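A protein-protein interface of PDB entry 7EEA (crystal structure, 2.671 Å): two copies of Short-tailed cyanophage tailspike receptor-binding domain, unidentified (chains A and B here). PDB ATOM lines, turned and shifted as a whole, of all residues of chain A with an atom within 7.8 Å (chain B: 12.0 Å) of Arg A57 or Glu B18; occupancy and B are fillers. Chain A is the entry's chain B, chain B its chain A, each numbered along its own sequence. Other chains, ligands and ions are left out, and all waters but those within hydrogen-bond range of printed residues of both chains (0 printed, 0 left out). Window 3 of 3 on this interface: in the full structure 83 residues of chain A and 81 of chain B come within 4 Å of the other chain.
The backbone NH (N) of Tyr B15 lies within hydrogen-bond range of the backbone carbonyl oxygen (O) of Arg B24, at 2.4 Å. OE1 of Glu B18 is in hydrogen-bond range of N of Gly B20, 2.5 Å away. SD of Met B29 is in hydrogen-bond range of NE of Arg B24, 3.7 Å away. The guanidinium group of Arg A57 is in salt-bridge range of the side-chain carboxylate of Glu A61, 2.9 Å away. N of Ile A63 lies within hydrogen-bond range of O of Ala A58, at 2.8 Å.
Among the printed residues, merely in contact across the chains: Leu A34 with Arg B17, Glu A38 with Ala B21, Glu A38 with Arg B24, Glu A38 with Met B29, Tyr A39 with Arg B17, Tyr A39 with Gly B20, Tyr A39 with Ala B21, Tyr A39 with Arg B22, Arg A57 with Glu B18 and Ile A63 with Arg B17.
Arg A57 touches just one residue of chain B: Glu B18 (3.4 Å). Glu B18 touches just these residues of chain A: Tyr A39 and Arg A57. No residue of chain B comes within 4 Å of Ala A53. No residue of chain B comes within 4 Å of Ala A54. No residue of chain B comes within 4 Å of Ala A56. No residue of chain B comes within 4 Å of Ala A58. No residue of chain B comes within 4 Å of Ser A60. Of chain B, only Arg B17 (2.5 Å) comes within 4 Å of Glu A61. Ile A63 touches just one residue of chain B: Arg B17 (3.4 Å). Printed residues of chain B within 4 Å of Glu A38: Tyr B15, Arg B17, Ala B21, Arg B22, Arg B24 and Met B29. Printed residues of chain B within 4 Å of Lys A31: Arg B17. Printed residues of chain A within 4 Å of Tyr B15: Glu A38. Of the printed residues of chain A, Ala B21 touches Glu A38 (3.6 Å) and Tyr A39 (3.8 Å). Printed residues of chain B within 4 Å of Tyr A39: Arg B17, Glu B18, Gly B20, Ala B21 and Arg B22. The nearest residue of chain B that does not touch Arg A57 is Arg B17 (4.02 Å).
Of the 20 printed residues of chain A, 7 touch a printed residue of chain B. Hydrophobic or aromatic side chains of chain A within 4 Å of the printed part of chain B: Leu A34, Tyr A39 and Ile A63. Among the printed residues, 16 pairs touch across the chains.
The side-chain carboxylate (OE1) of Glu A38 lies within hydrogen-bond range of the side-chain hydroxyl (OH) of Tyr B15 (2.9 Å). The backbone carbonyl oxygen (O) of Lys A31 lies within hydrogen-bond range of the guanidinium group (NH1) of Arg B17, at 2.8 Å. The side-chain carboxylate of Glu A38 is in salt-bridge range of the guanidinium group of Arg B17 (3.1 Å). The side-chain carboxylate of Glu A61 is in salt-bridge range of the guanidinium group of Arg B17 (2.5 Å). OH of Tyr A39 is in hydrogen-bond range of OE2 of Glu B18, 2.7 Å away. The backbone NH (N) of Arg B22 is in hydrogen-bond range of the backbone carbonyl oxygen (O) of Glu A38.
No position is printed for both chains. Of the 16 pairs that touch across the chains among the printed residues, none has its exchanged pair printed and touching as well.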
ATOM      1  N   LYS A  31     -18.662   4.424 -36.018  1.00  0.00           N
ATOM      2  CA  LYS A  31     -18.022   3.278 -35.382  1.00  0.00           C
ATOM      3  C   LYS A  31     -17.360   2.332 -36.376  1.00  0.00           C
ATOM      4  O   LYS A  31     -16.558   1.490 -35.956  1.00  0.00           O
ATOM      5  CB  LYS A  31     -19.039   2.512 -34.534  1.00  0.00           C
ATOM      6  CG  LYS A  31     -19.166   3.034 -33.109  1.00  0.00           C
ATOM      7  CD  LYS A  31     -20.620   3.206 -32.690  1.00  0.00           C
ATOM      8  CE  LYS A  31     -21.485   2.053 -33.171  1.00  0.00           C
ATOM      9  NZ  LYS A  31     -22.526   1.692 -32.169  1.00  0.00           N
ATOM     10  N   LEU A  34     -12.150   4.374 -36.606  1.00  0.00           N
ATOM     11  CA  LEU A  34     -11.706   4.772 -35.270  1.00  0.00           C
ATOM     12  C   LEU A  34     -10.961   6.097 -35.393  1.00  0.00           C
ATOM     13  O   LEU A  34      -9.810   6.130 -35.838  1.00  0.00           O
ATOM     14  CB  LEU A  34     -10.836   3.703 -34.621  1.00  0.00           C
ATOM     15  CG  LEU A  34     -10.583   3.941 -33.130  1.00  0.00           C
ATOM     16  CD1 LEU A  34     -10.853   2.680 -32.326  1.00  0.00           C
ATOM     17  CD2 LEU A  34      -9.169   4.442 -32.887  1.00  0.00           C
ATOM     18  N   GLU A  38     -11.655  10.811 -30.922  1.00  0.00           N
ATOM     19  CA  GLU A  38     -12.650  10.244 -30.018  1.00  0.00           C
ATOM     20  C   GLU A  38     -12.069   9.992 -28.637  1.00  0.00           C
ATOM     21  O   GLU A  38     -12.819   9.933 -27.657  1.00  0.00           O
ATOM     22  CB  GLU A  38     -13.205   8.935 -30.585  1.00  0.00           C
ATOM     23  CG  GLU A  38     -13.849   9.081 -31.949  1.00  0.00           C
ATOM     24  CD  GLU A  38     -14.330   7.760 -32.514  1.00  0.00           C
ATOM     25  OE1 GLU A  38     -15.158   7.092 -31.857  1.00  0.00           O
ATOM     26  OE2 GLU A  38     -13.882   7.393 -33.621  1.00  0.00           O
ATOM     27  N   TYR A  39     -10.749   9.841 -28.542  1.00  0.00           N
ATOM     28  CA  TYR A  39     -10.070   9.646 -27.271  1.00  0.00           C
ATOM     29  C   TYR A  39      -9.124  10.779 -26.906  1.00  0.00           C
ATOM     30  O   TYR A  39      -9.005  11.107 -25.723  1.00  0.00           O
ATOM     31  CB  TYR A  39      -9.288   8.325 -27.284  1.00  0.00           C
ATOM     32  CG  TYR A  39     -10.191   7.114 -27.243  1.00  0.00           C
ATOM     33  CD1 TYR A  39     -10.699   6.559 -28.412  1.00  0.00           C
ATOM     34  CD2 TYR A  39     -10.555   6.538 -26.032  1.00  0.00           C
ATOM     35  CE1 TYR A  39     -11.534   5.460 -28.375  1.00  0.00           C
ATOM     36  CE2 TYR A  39     -11.389   5.442 -25.986  1.00  0.00           C
ATOM     37  CZ  TYR A  39     -11.877   4.907 -27.158  1.00  0.00           C
ATOM     38  OH  TYR A  39     -12.708   3.813 -27.106  1.00  0.00           O
ATOM     39  N   ALA A  50      -4.780   8.603 -23.136  1.00  0.00           N
ATOM     40  CA  ALA A  50      -5.861   8.573 -24.116  1.00  0.00           C
ATOM     41  C   ALA A  50      -5.429   7.864 -25.393  1.00  0.00           C
ATOM     42  O   ALA A  50      -6.187   7.064 -25.953  1.00  0.00           O
ATOM     43  CB  ALA A  50      -6.329   9.995 -24.419  1.00  0.00           C
ATOM     44  N   PHE A  51      -4.212   8.148 -25.866  1.00  0.00           N
ATOM     45  CA  PHE A  51      -3.700   7.486 -27.061  1.00  0.00           C
ATOM     46  C   PHE A  51      -3.598   5.980 -26.854  1.00  0.00           C
ATOM     47  O   PHE A  51      -3.960   5.198 -27.741  1.00  0.00           O
ATOM     48  CB  PHE A  51      -2.336   8.074 -27.431  1.00  0.00           C
ATOM     49  CG  PHE A  51      -2.063   8.109 -28.909  1.00  0.00           C
ATOM     50  CD1 PHE A  51      -2.332   7.012 -29.710  1.00  0.00           C
ATOM     51  CD2 PHE A  51      -1.517   9.241 -29.494  1.00  0.00           C
ATOM     52  CE1 PHE A  51      -2.071   7.048 -31.069  1.00  0.00           C
ATOM     53  CE2 PHE A  51      -1.254   9.281 -30.850  1.00  0.00           C
ATOM     54  CZ  PHE A  51      -1.531   8.185 -31.639  1.00  0.00           C
ATOM     55  N   ASN A  52      -3.109   5.555 -25.685  1.00  0.00           N
ATOM     56  CA  ASN A  52      -3.005   4.128 -25.401  1.00  0.00           C
ATOM     57  C   ASN A  52      -4.374   3.463 -25.410  1.00  0.00           C
ATOM     58  O   ASN A  52      -4.510   2.309 -25.833  1.00  0.00           O
ATOM     59  CB  ASN A  52      -2.316   3.911 -24.054  1.00  0.00           C
ATOM     60  CG  ASN A  52      -0.816   3.733 -24.187  1.00  0.00           C
ATOM     61  OD1 ASN A  52      -0.337   3.066 -25.106  1.00  0.00           O
ATOM     62  ND2 ASN A  52      -0.064   4.328 -23.267  1.00  0.00           N
ATOM     63  N   ALA A  53      -5.404   4.180 -24.953  1.00  0.00           N
ATOM     64  CA  ALA A  53      -6.750   3.618 -24.934  1.00  0.00           C
ATOM     65  C   ALA A  53      -7.303   3.461 -26.344  1.00  0.00           C
ATOM     66  O   ALA A  53      -8.003   2.484 -26.637  1.00  0.00           O
ATOM     67  CB  ALA A  53      -7.675   4.495 -24.087  1.00  0.00           C
ATOM     68  N   ALA A  54      -6.996   4.410 -27.232  1.00  0.00           N
ATOM     69  CA  ALA A  54      -7.482   4.320 -28.605  1.00  0.00           C
ATOM     70  C   ALA A  54      -6.818   3.169 -29.349  1.00  0.00           C
ATOM     71  O   ALA A  54      -7.471   2.479 -30.141  1.00  0.00           O
ATOM     72  CB  ALA A  54      -7.246   5.640 -29.337  1.00  0.00           C
ATOM     73  N   ILE A  55      -5.522   2.956 -29.116  1.00  0.00           N
ATOM     74  CA  ILE A  55      -4.839   1.809 -29.710  1.00  0.00           C
ATOM     75  C   ILE A  55      -5.479   0.515 -29.229  1.00  0.00           C
ATOM     76  O   ILE A  55      -5.771  -0.389 -30.022  1.00  0.00           O
ATOM     77  CB  ILE A  55      -3.335   1.847 -29.382  1.00  0.00           C
ATOM     78  CG1 ILE A  55      -2.698   3.121 -29.940  1.00  0.00           C
ATOM     79  CG2 ILE A  55      -2.639   0.618 -29.935  1.00  0.00           C
ATOM     80  CD1 ILE A  55      -1.303   3.384 -29.417  1.00  0.00           C
ATOM     81  N   ALA A  56      -5.727   0.418 -27.920  1.00  0.00           N
ATOM     82  CA  ALA A  56      -6.327  -0.789 -27.363  1.00  0.00           C
ATOM     83  C   ALA A  56      -7.767  -0.969 -27.823  1.00  0.00           C
ATOM     84  O   ALA A  56      -8.233  -2.107 -27.960  1.00  0.00           O
ATOM     85  CB  ALA A  56      -6.255  -0.755 -25.836  1.00  0.00           C
ATOM     86  N   ARG A  57      -8.487   0.128 -28.068  1.00  0.00           N
ATOM     87  CA  ARG A  57      -9.859   0.003 -28.548  1.00  0.00           C
ATOM     88  C   ARG A  57      -9.895  -0.544 -29.970  1.00  0.00           C
ATOM     89  O   ARG A  57     -10.746  -1.377 -30.298  1.00  0.00           O
ATOM     90  CB  ARG A  57     -10.577   1.349 -28.472  1.00  0.00           C
ATOM     91  CG  ARG A  57     -12.062   1.267 -28.789  1.00  0.00           C
ATOM     92  CD  ARG A  57     -12.819   0.485 -27.723  1.00  0.00           C
ATOM     93  NE  ARG A  57     -14.181   0.168 -28.147  1.00  0.00           N
ATOM     94  CZ  ARG A  57     -15.095  -0.405 -27.367  1.00  0.00           C
ATOM     95  NH1 ARG A  57     -14.796  -0.727 -26.115  1.00  0.00           N
ATOM     96  NH2 ARG A  57     -16.310  -0.657 -27.838  1.00  0.00           N
ATOM     97  N   ALA A  58      -8.978  -0.084 -30.824  1.00  0.00           N
ATOM     98  CA  ALA A  58      -8.898  -0.618 -32.180  1.00  0.00           C
ATOM     99  C   ALA A  58      -8.598  -2.109 -32.162  1.00  0.00           C
ATOM    100  O   ALA A  58      -9.197  -2.881 -32.920  1.00  0.00           O
ATOM    101  CB  ALA A  58      -7.834   0.134 -32.980  1.00  0.00           C
ATOM    102  N   VAL A  59      -7.673  -2.531 -31.295  1.00  0.00           N
ATOM    103  CA  VAL A  59      -7.353  -3.949 -31.170  1.00  0.00           C
ATOM    104  C   VAL A  59      -8.570  -4.729 -30.692  1.00  0.00           C
ATOM    105  O   VAL A  59      -8.846  -5.836 -31.171  1.00  0.00           O
ATOM    106  CB  VAL A  59      -6.153  -4.140 -30.223  1.00  0.00           C
ATOM    107  CG1 VAL A  59      -5.819  -5.616 -30.078  1.00  0.00           C
ATOM    108  CG2 VAL A  59      -4.953  -3.362 -30.728  1.00  0.00           C
ATOM    109  N   SER A  60      -9.323  -4.161 -29.746  1.00  0.00           N
ATOM    110  CA  SER A  60     -10.471  -4.872 -29.193  1.00  0.00           C
ATOM    111  C   SER A  60     -11.610  -4.967 -30.202  1.00  0.00           C
ATOM    112  O   SER A  60     -12.284  -6.001 -30.288  1.00  0.00           O
ATOM    113  CB  SER A  60     -10.942  -4.185 -27.913  1.00  0.00           C
ATOM    114  OG  SER A  60      -9.949  -4.267 -26.903  1.00  0.00           O
ATOM    115  N   GLU A  61     -11.840  -3.906 -30.975  1.00  0.00           N
ATOM    116  CA  GLU A  61     -12.901  -3.917 -31.974  1.00  0.00           C
ATOM    117  C   GLU A  61     -12.485  -4.588 -33.278  1.00  0.00           C
ATOM    118  O   GLU A  61     -13.327  -4.748 -34.167  1.00  0.00           O
ATOM    119  CB  GLU A  61     -13.373  -2.487 -32.262  1.00  0.00           C
ATOM    120  CG  GLU A  61     -14.322  -1.915 -31.217  1.00  0.00           C
ATOM    121  CD  GLU A  61     -14.983  -0.624 -31.669  1.00  0.00           C
ATOM    122  OE1 GLU A  61     -14.959   0.362 -30.900  1.00  0.00           O
ATOM    123  OE2 GLU A  61     -15.532  -0.595 -32.793  1.00  0.00           O
ATOM    124  N   GLY A  62     -11.221  -4.983 -33.411  1.00  0.00           N
ATOM    125  CA  GLY A  62     -10.754  -5.579 -34.649  1.00  0.00           C
ATOM    126  C   GLY A  62     -10.602  -4.597 -35.787  1.00  0.00           C
ATOM    127  O   GLY A  62     -10.844  -4.954 -36.943  1.00  0.00           O
ATOM    128  N   ILE A  63     -10.203  -3.362 -35.489  1.00  0.00           N
ATOM    129  CA  ILE A  63     -10.075  -2.299 -36.477  1.00  0.00           C
ATOM    130  C   ILE A  63      -8.596  -2.032 -36.711  1.00  0.00           C
ATOM    131  O   ILE A  63      -7.804  -2.003 -35.762  1.00  0.00           O
ATOM    132  CB  ILE A  63     -10.806  -1.022 -36.015  1.00  0.00           C
ATOM    133  CG1 ILE A  63     -12.320  -1.217 -36.097  1.00  0.00           C
ATOM    134  CG2 ILE A  63     -10.380   0.184 -36.838  1.00  0.00           C
ATOM    135  CD1 ILE A  63     -13.112   0.036 -35.796  1.00  0.00           C
ATOM    136  N   ILE A  66      -6.301   3.781 -37.622  1.00  0.00           N
ATOM    137  CA  ILE A  66      -6.584   4.804 -36.623  1.00  0.00           C
ATOM    138  C   ILE A  66      -6.338   6.148 -37.293  1.00  0.00           C
ATOM    139  O   ILE A  66      -5.189   6.495 -37.596  1.00  0.00           O
ATOM    140  CB  ILE A  66      -5.720   4.644 -35.365  1.00  0.00           C
ATOM    141  CG1 ILE A  66      -5.980   3.287 -34.705  1.00  0.00           C
ATOM    142  CG2 ILE A  66      -5.984   5.778 -34.387  1.00  0.00           C
ATOM    143  CD1 ILE A  66      -5.377   3.153 -33.322  1.00  0.00           C
ATOM    144  N   LEU A  85      -2.318  -2.682 -37.419  1.00  0.00           N
ATOM    145  CA  LEU A  85      -2.740  -1.309 -37.174  1.00  0.00           C
ATOM    146  C   LEU A  85      -2.125  -0.336 -38.174  1.00  0.00           C
ATOM    147  O   LEU A  85      -0.941  -0.429 -38.516  1.00  0.00           O
ATOM    148  CB  LEU A  85      -2.387  -0.899 -35.746  1.00  0.00           C
ATOM    149  CG  LEU A  85      -3.227  -1.623 -34.690  1.00  0.00           C
ATOM    150  CD1 LEU A  85      -2.790  -1.252 -33.288  1.00  0.00           C
ATOM    151  CD2 LEU A  85      -4.704  -1.327 -34.892  1.00  0.00           C
ATOM    152  N   GLY B  14     -25.267  14.255 -29.137  1.00  0.00           N
ATOM    153  CA  GLY B  14     -24.096  13.664 -28.523  1.00  0.00           C
ATOM    154  C   GLY B  14     -23.729  12.335 -29.154  1.00  0.00           C
ATOM    155  O   GLY B  14     -24.582  11.573 -29.608  1.00  0.00           O
ATOM    156  N   TYR B  15     -22.428  12.057 -29.183  1.00  0.00           N
ATOM    157  CA  TYR B  15     -21.921  10.811 -29.737  1.00  0.00           C
ATOM    158  C   TYR B  15     -20.782  10.291 -28.873  1.00  0.00           C
ATOM    159  O   TYR B  15     -19.926  11.061 -28.428  1.00  0.00           O
ATOM    160  CB  TYR B  15     -21.434  10.984 -31.180  1.00  0.00           C
ATOM    161  CG  TYR B  15     -20.488   9.891 -31.610  1.00  0.00           C
ATOM    162  CD1 TYR B  15     -20.957   8.613 -31.885  1.00  0.00           C
ATOM    163  CD2 TYR B  15     -19.125  10.128 -31.723  1.00  0.00           C
ATOM    164  CE1 TYR B  15     -20.095   7.603 -32.270  1.00  0.00           C
ATOM    165  CE2 TYR B  15     -18.257   9.126 -32.105  1.00  0.00           C
ATOM    166  CZ  TYR B  15     -18.747   7.866 -32.378  1.00  0.00           C
ATOM    167  OH  TYR B  15     -17.884   6.867 -32.762  1.00  0.00           O
ATOM    168  N   LYS B  16     -20.773   8.979 -28.652  1.00  0.00           N
ATOM    169  CA  LYS B  16     -19.750   8.339 -27.839  1.00  0.00           C
ATOM    170  C   LYS B  16     -19.558   6.914 -28.331  1.00  0.00           C
ATOM    171  O   LYS B  16     -20.534   6.177 -28.498  1.00  0.00           O
ATOM    172  CB  LYS B  16     -20.140   8.348 -26.359  1.00  0.00           C
ATOM    173  CG  LYS B  16     -18.974   8.485 -25.400  1.00  0.00           C
ATOM    174  CD  LYS B  16     -19.465   8.586 -23.968  1.00  0.00           C
ATOM    175  CE  LYS B  16     -18.326   8.862 -23.004  1.00  0.00           C
ATOM    176  NZ  LYS B  16     -18.808   9.045 -21.608  1.00  0.00           N
ATOM    177  N   ARG B  17     -18.302   6.535 -28.571  1.00  0.00           N
ATOM    178  CA  ARG B  17     -18.001   5.171 -28.994  1.00  0.00           C
ATOM    179  C   ARG B  17     -18.317   4.174 -27.885  1.00  0.00           C
ATOM    180  O   ARG B  17     -19.088   3.226 -28.079  1.00  0.00           O
ATOM    181  CB  ARG B  17     -16.532   5.073 -29.407  1.00  0.00           C
ATOM    182  CG  ARG B  17     -16.098   3.695 -29.844  1.00  0.00           C
ATOM    183  CD  ARG B  17     -14.729   3.744 -30.499  1.00  0.00           C
ATOM    184  NE  ARG B  17     -14.625   2.783 -31.591  1.00  0.00           N
ATOM    185  CZ  ARG B  17     -14.954   3.048 -32.850  1.00  0.00           C
ATOM    186  NH1 ARG B  17     -14.832   2.112 -33.781  1.00  0.00           N
ATOM    187  NH2 ARG B  17     -15.404   4.251 -33.178  1.00  0.00           N
ATOM    188  N   GLU B  18     -17.716   4.374 -26.716  1.00  0.00           N
ATOM    189  CA  GLU B  18     -17.997   3.574 -25.535  1.00  0.00           C
ATOM    190  C   GLU B  18     -17.814   4.471 -24.317  1.00  0.00           C
ATOM    191  O   GLU B  18     -17.430   5.638 -24.437  1.00  0.00           O
ATOM    192  CB  GLU B  18     -17.099   2.335 -25.482  1.00  0.00           C
ATOM    193  CG  GLU B  18     -15.642   2.615 -25.802  1.00  0.00           C
ATOM    194  CD  GLU B  18     -14.800   2.783 -24.556  1.00  0.00           C
ATOM    195  OE1 GLU B  18     -15.356   2.648 -23.446  1.00  0.00           O
ATOM    196  OE2 GLU B  18     -13.585   3.046 -24.686  1.00  0.00           O
ATOM    197  N   SER B  19     -18.092   3.916 -23.134  1.00  0.00           N
ATOM    198  CA  SER B  19     -18.080   4.725 -21.917  1.00  0.00           C
ATOM    199  C   SER B  19     -16.724   5.376 -21.676  1.00  0.00           C
ATOM    200  O   SER B  19     -16.659   6.504 -21.171  1.00  0.00           O
ATOM    201  CB  SER B  19     -18.478   3.868 -20.714  1.00  0.00           C
ATOM    202  OG  SER B  19     -17.664   2.710 -20.617  1.00  0.00           O
ATOM    203  N   GLY B  20     -15.636   4.699 -22.038  1.00  0.00           N
ATOM    204  CA  GLY B  20     -14.302   5.214 -21.805  1.00  0.00           C
ATOM    205  C   GLY B  20     -13.813   6.266 -22.776  1.00  0.00           C
ATOM    206  O   GLY B  20     -12.680   6.735 -22.637  1.00  0.00           O
ATOM    207  N   ALA B  21     -14.625   6.659 -23.753  1.00  0.00           N
ATOM    208  CA  ALA B  21     -14.212   7.640 -24.744  1.00  0.00           C
ATOM    209  C   ALA B  21     -14.609   9.048 -24.299  1.00  0.00           C
ATOM    210  O   ALA B  21     -15.172   9.256 -23.222  1.00  0.00           O
ATOM    211  CB  ALA B  21     -14.813   7.302 -26.108  1.00  0.00           C
ATOM    212  N   ARG B  22     -14.301  10.034 -25.138  1.00  0.00           N
ATOM    213  CA  ARG B  22     -14.715  11.404 -24.877  1.00  0.00           C
ATOM    214  C   ARG B  22     -16.145  11.617 -25.348  1.00  0.00           C
ATOM    215  O   ARG B  22     -16.570  11.055 -26.361  1.00  0.00           O
ATOM    216  CB  ARG B  22     -13.790  12.393 -25.584  1.00  0.00           C
ATOM    217  CG  ARG B  22     -12.321  12.265 -25.238  1.00  0.00           C
ATOM    218  CD  ARG B  22     -11.486  13.123 -26.172  1.00  0.00           C
ATOM    219  NE  ARG B  22     -11.785  14.544 -26.017  1.00  0.00           N
ATOM    220  CZ  ARG B  22     -11.895  15.398 -27.030  1.00  0.00           C
ATOM    221  NH1 ARG B  22     -11.732  14.974 -28.276  1.00  0.00           N
ATOM    222  NH2 ARG B  22     -12.169  16.676 -26.799  1.00  0.00           N
ATOM    223  N   LEU B  23     -16.890  12.435 -24.609  1.00  0.00           N
ATOM    224  CA  LEU B  23     -18.228  12.819 -25.037  1.00  0.00           C
ATOM    225  C   LEU B  23     -18.110  13.900 -26.100  1.00  0.00           C
ATOM    226  O   LEU B  23     -17.613  14.997 -25.826  1.00  0.00           O
ATOM    227  CB  LEU B  23     -19.063  13.314 -23.860  1.00  0.00           C
ATOM    228  CG  LEU B  23     -20.523  13.599 -24.229  1.00  0.00           C
ATOM    229  CD1 LEU B  23     -21.198  12.338 -24.751  1.00  0.00           C
ATOM    230  CD2 LEU B  23     -21.287  14.174 -23.047  1.00  0.00           C
ATOM    231  N   ARG B  24     -18.562  13.591 -27.311  1.00  0.00           N
ATOM    232  CA  ARG B  24     -18.450  14.503 -28.435  1.00  0.00           C
ATOM    233  C   ARG B  24     -19.788  14.591 -29.155  1.00  0.00           C
ATOM    234  O   ARG B  24     -20.674  13.751 -28.976  1.00  0.00           O
ATOM    235  CB  ARG B  24     -17.347  14.057 -29.408  1.00  0.00           C
ATOM    236  CG  ARG B  24     -15.937  14.338 -28.905  1.00  0.00           C
ATOM    237  CD  ARG B  24     -14.901  13.441 -29.564  1.00  0.00           C
ATOM    238  NE  ARG B  24     -14.795  13.669 -31.002  1.00  0.00           N
ATOM    239  CZ  ARG B  24     -14.144  14.690 -31.553  1.00  0.00           C
ATOM    240  NH1 ARG B  24     -13.539  15.588 -30.787  1.00  0.00           N
ATOM    241  NH2 ARG B  24     -14.097  14.813 -32.872  1.00  0.00           N
ATOM    242  N   THR B  25     -19.924  15.632 -29.965  1.00  0.00           N
ATOM    243  CA  THR B  25     -21.089  15.794 -30.815  1.00  0.00           C
ATOM    244  C   THR B  25     -20.843  15.124 -32.163  1.00  0.00           C
ATOM    245  O   THR B  25     -19.715  14.782 -32.520  1.00  0.00           O
ATOM    246  CB  THR B  25     -21.410  17.277 -31.004  1.00  0.00           C
ATOM    247  OG1 THR B  25     -20.503  17.845 -31.957  1.00  0.00           O
ATOM    248  CG2 THR B  25     -21.265  18.018 -29.687  1.00  0.00           C
ATOM    249  N   MET B  29     -17.250  15.228 -34.814  1.00  0.00           N
ATOM    250  CA  MET B  29     -16.668  14.204 -35.674  1.00  0.00           C
ATOM    251  C   MET B  29     -16.438  14.723 -37.084  1.00  0.00           C
ATOM    252  O   MET B  29     -15.487  14.300 -37.754  1.00  0.00           O
ATOM    253  CB  MET B  29     -17.571  12.971 -35.701  1.00  0.00           C
ATOM    254  CG  MET B  29     -17.828  12.362 -34.334  1.00  0.00           C
ATOM    255  SD  MET B  29     -16.355  11.592 -33.640  1.00  0.00           S
ATOM    256  CE  MET B  29     -16.144  10.208 -34.757  1.00  0.00           C
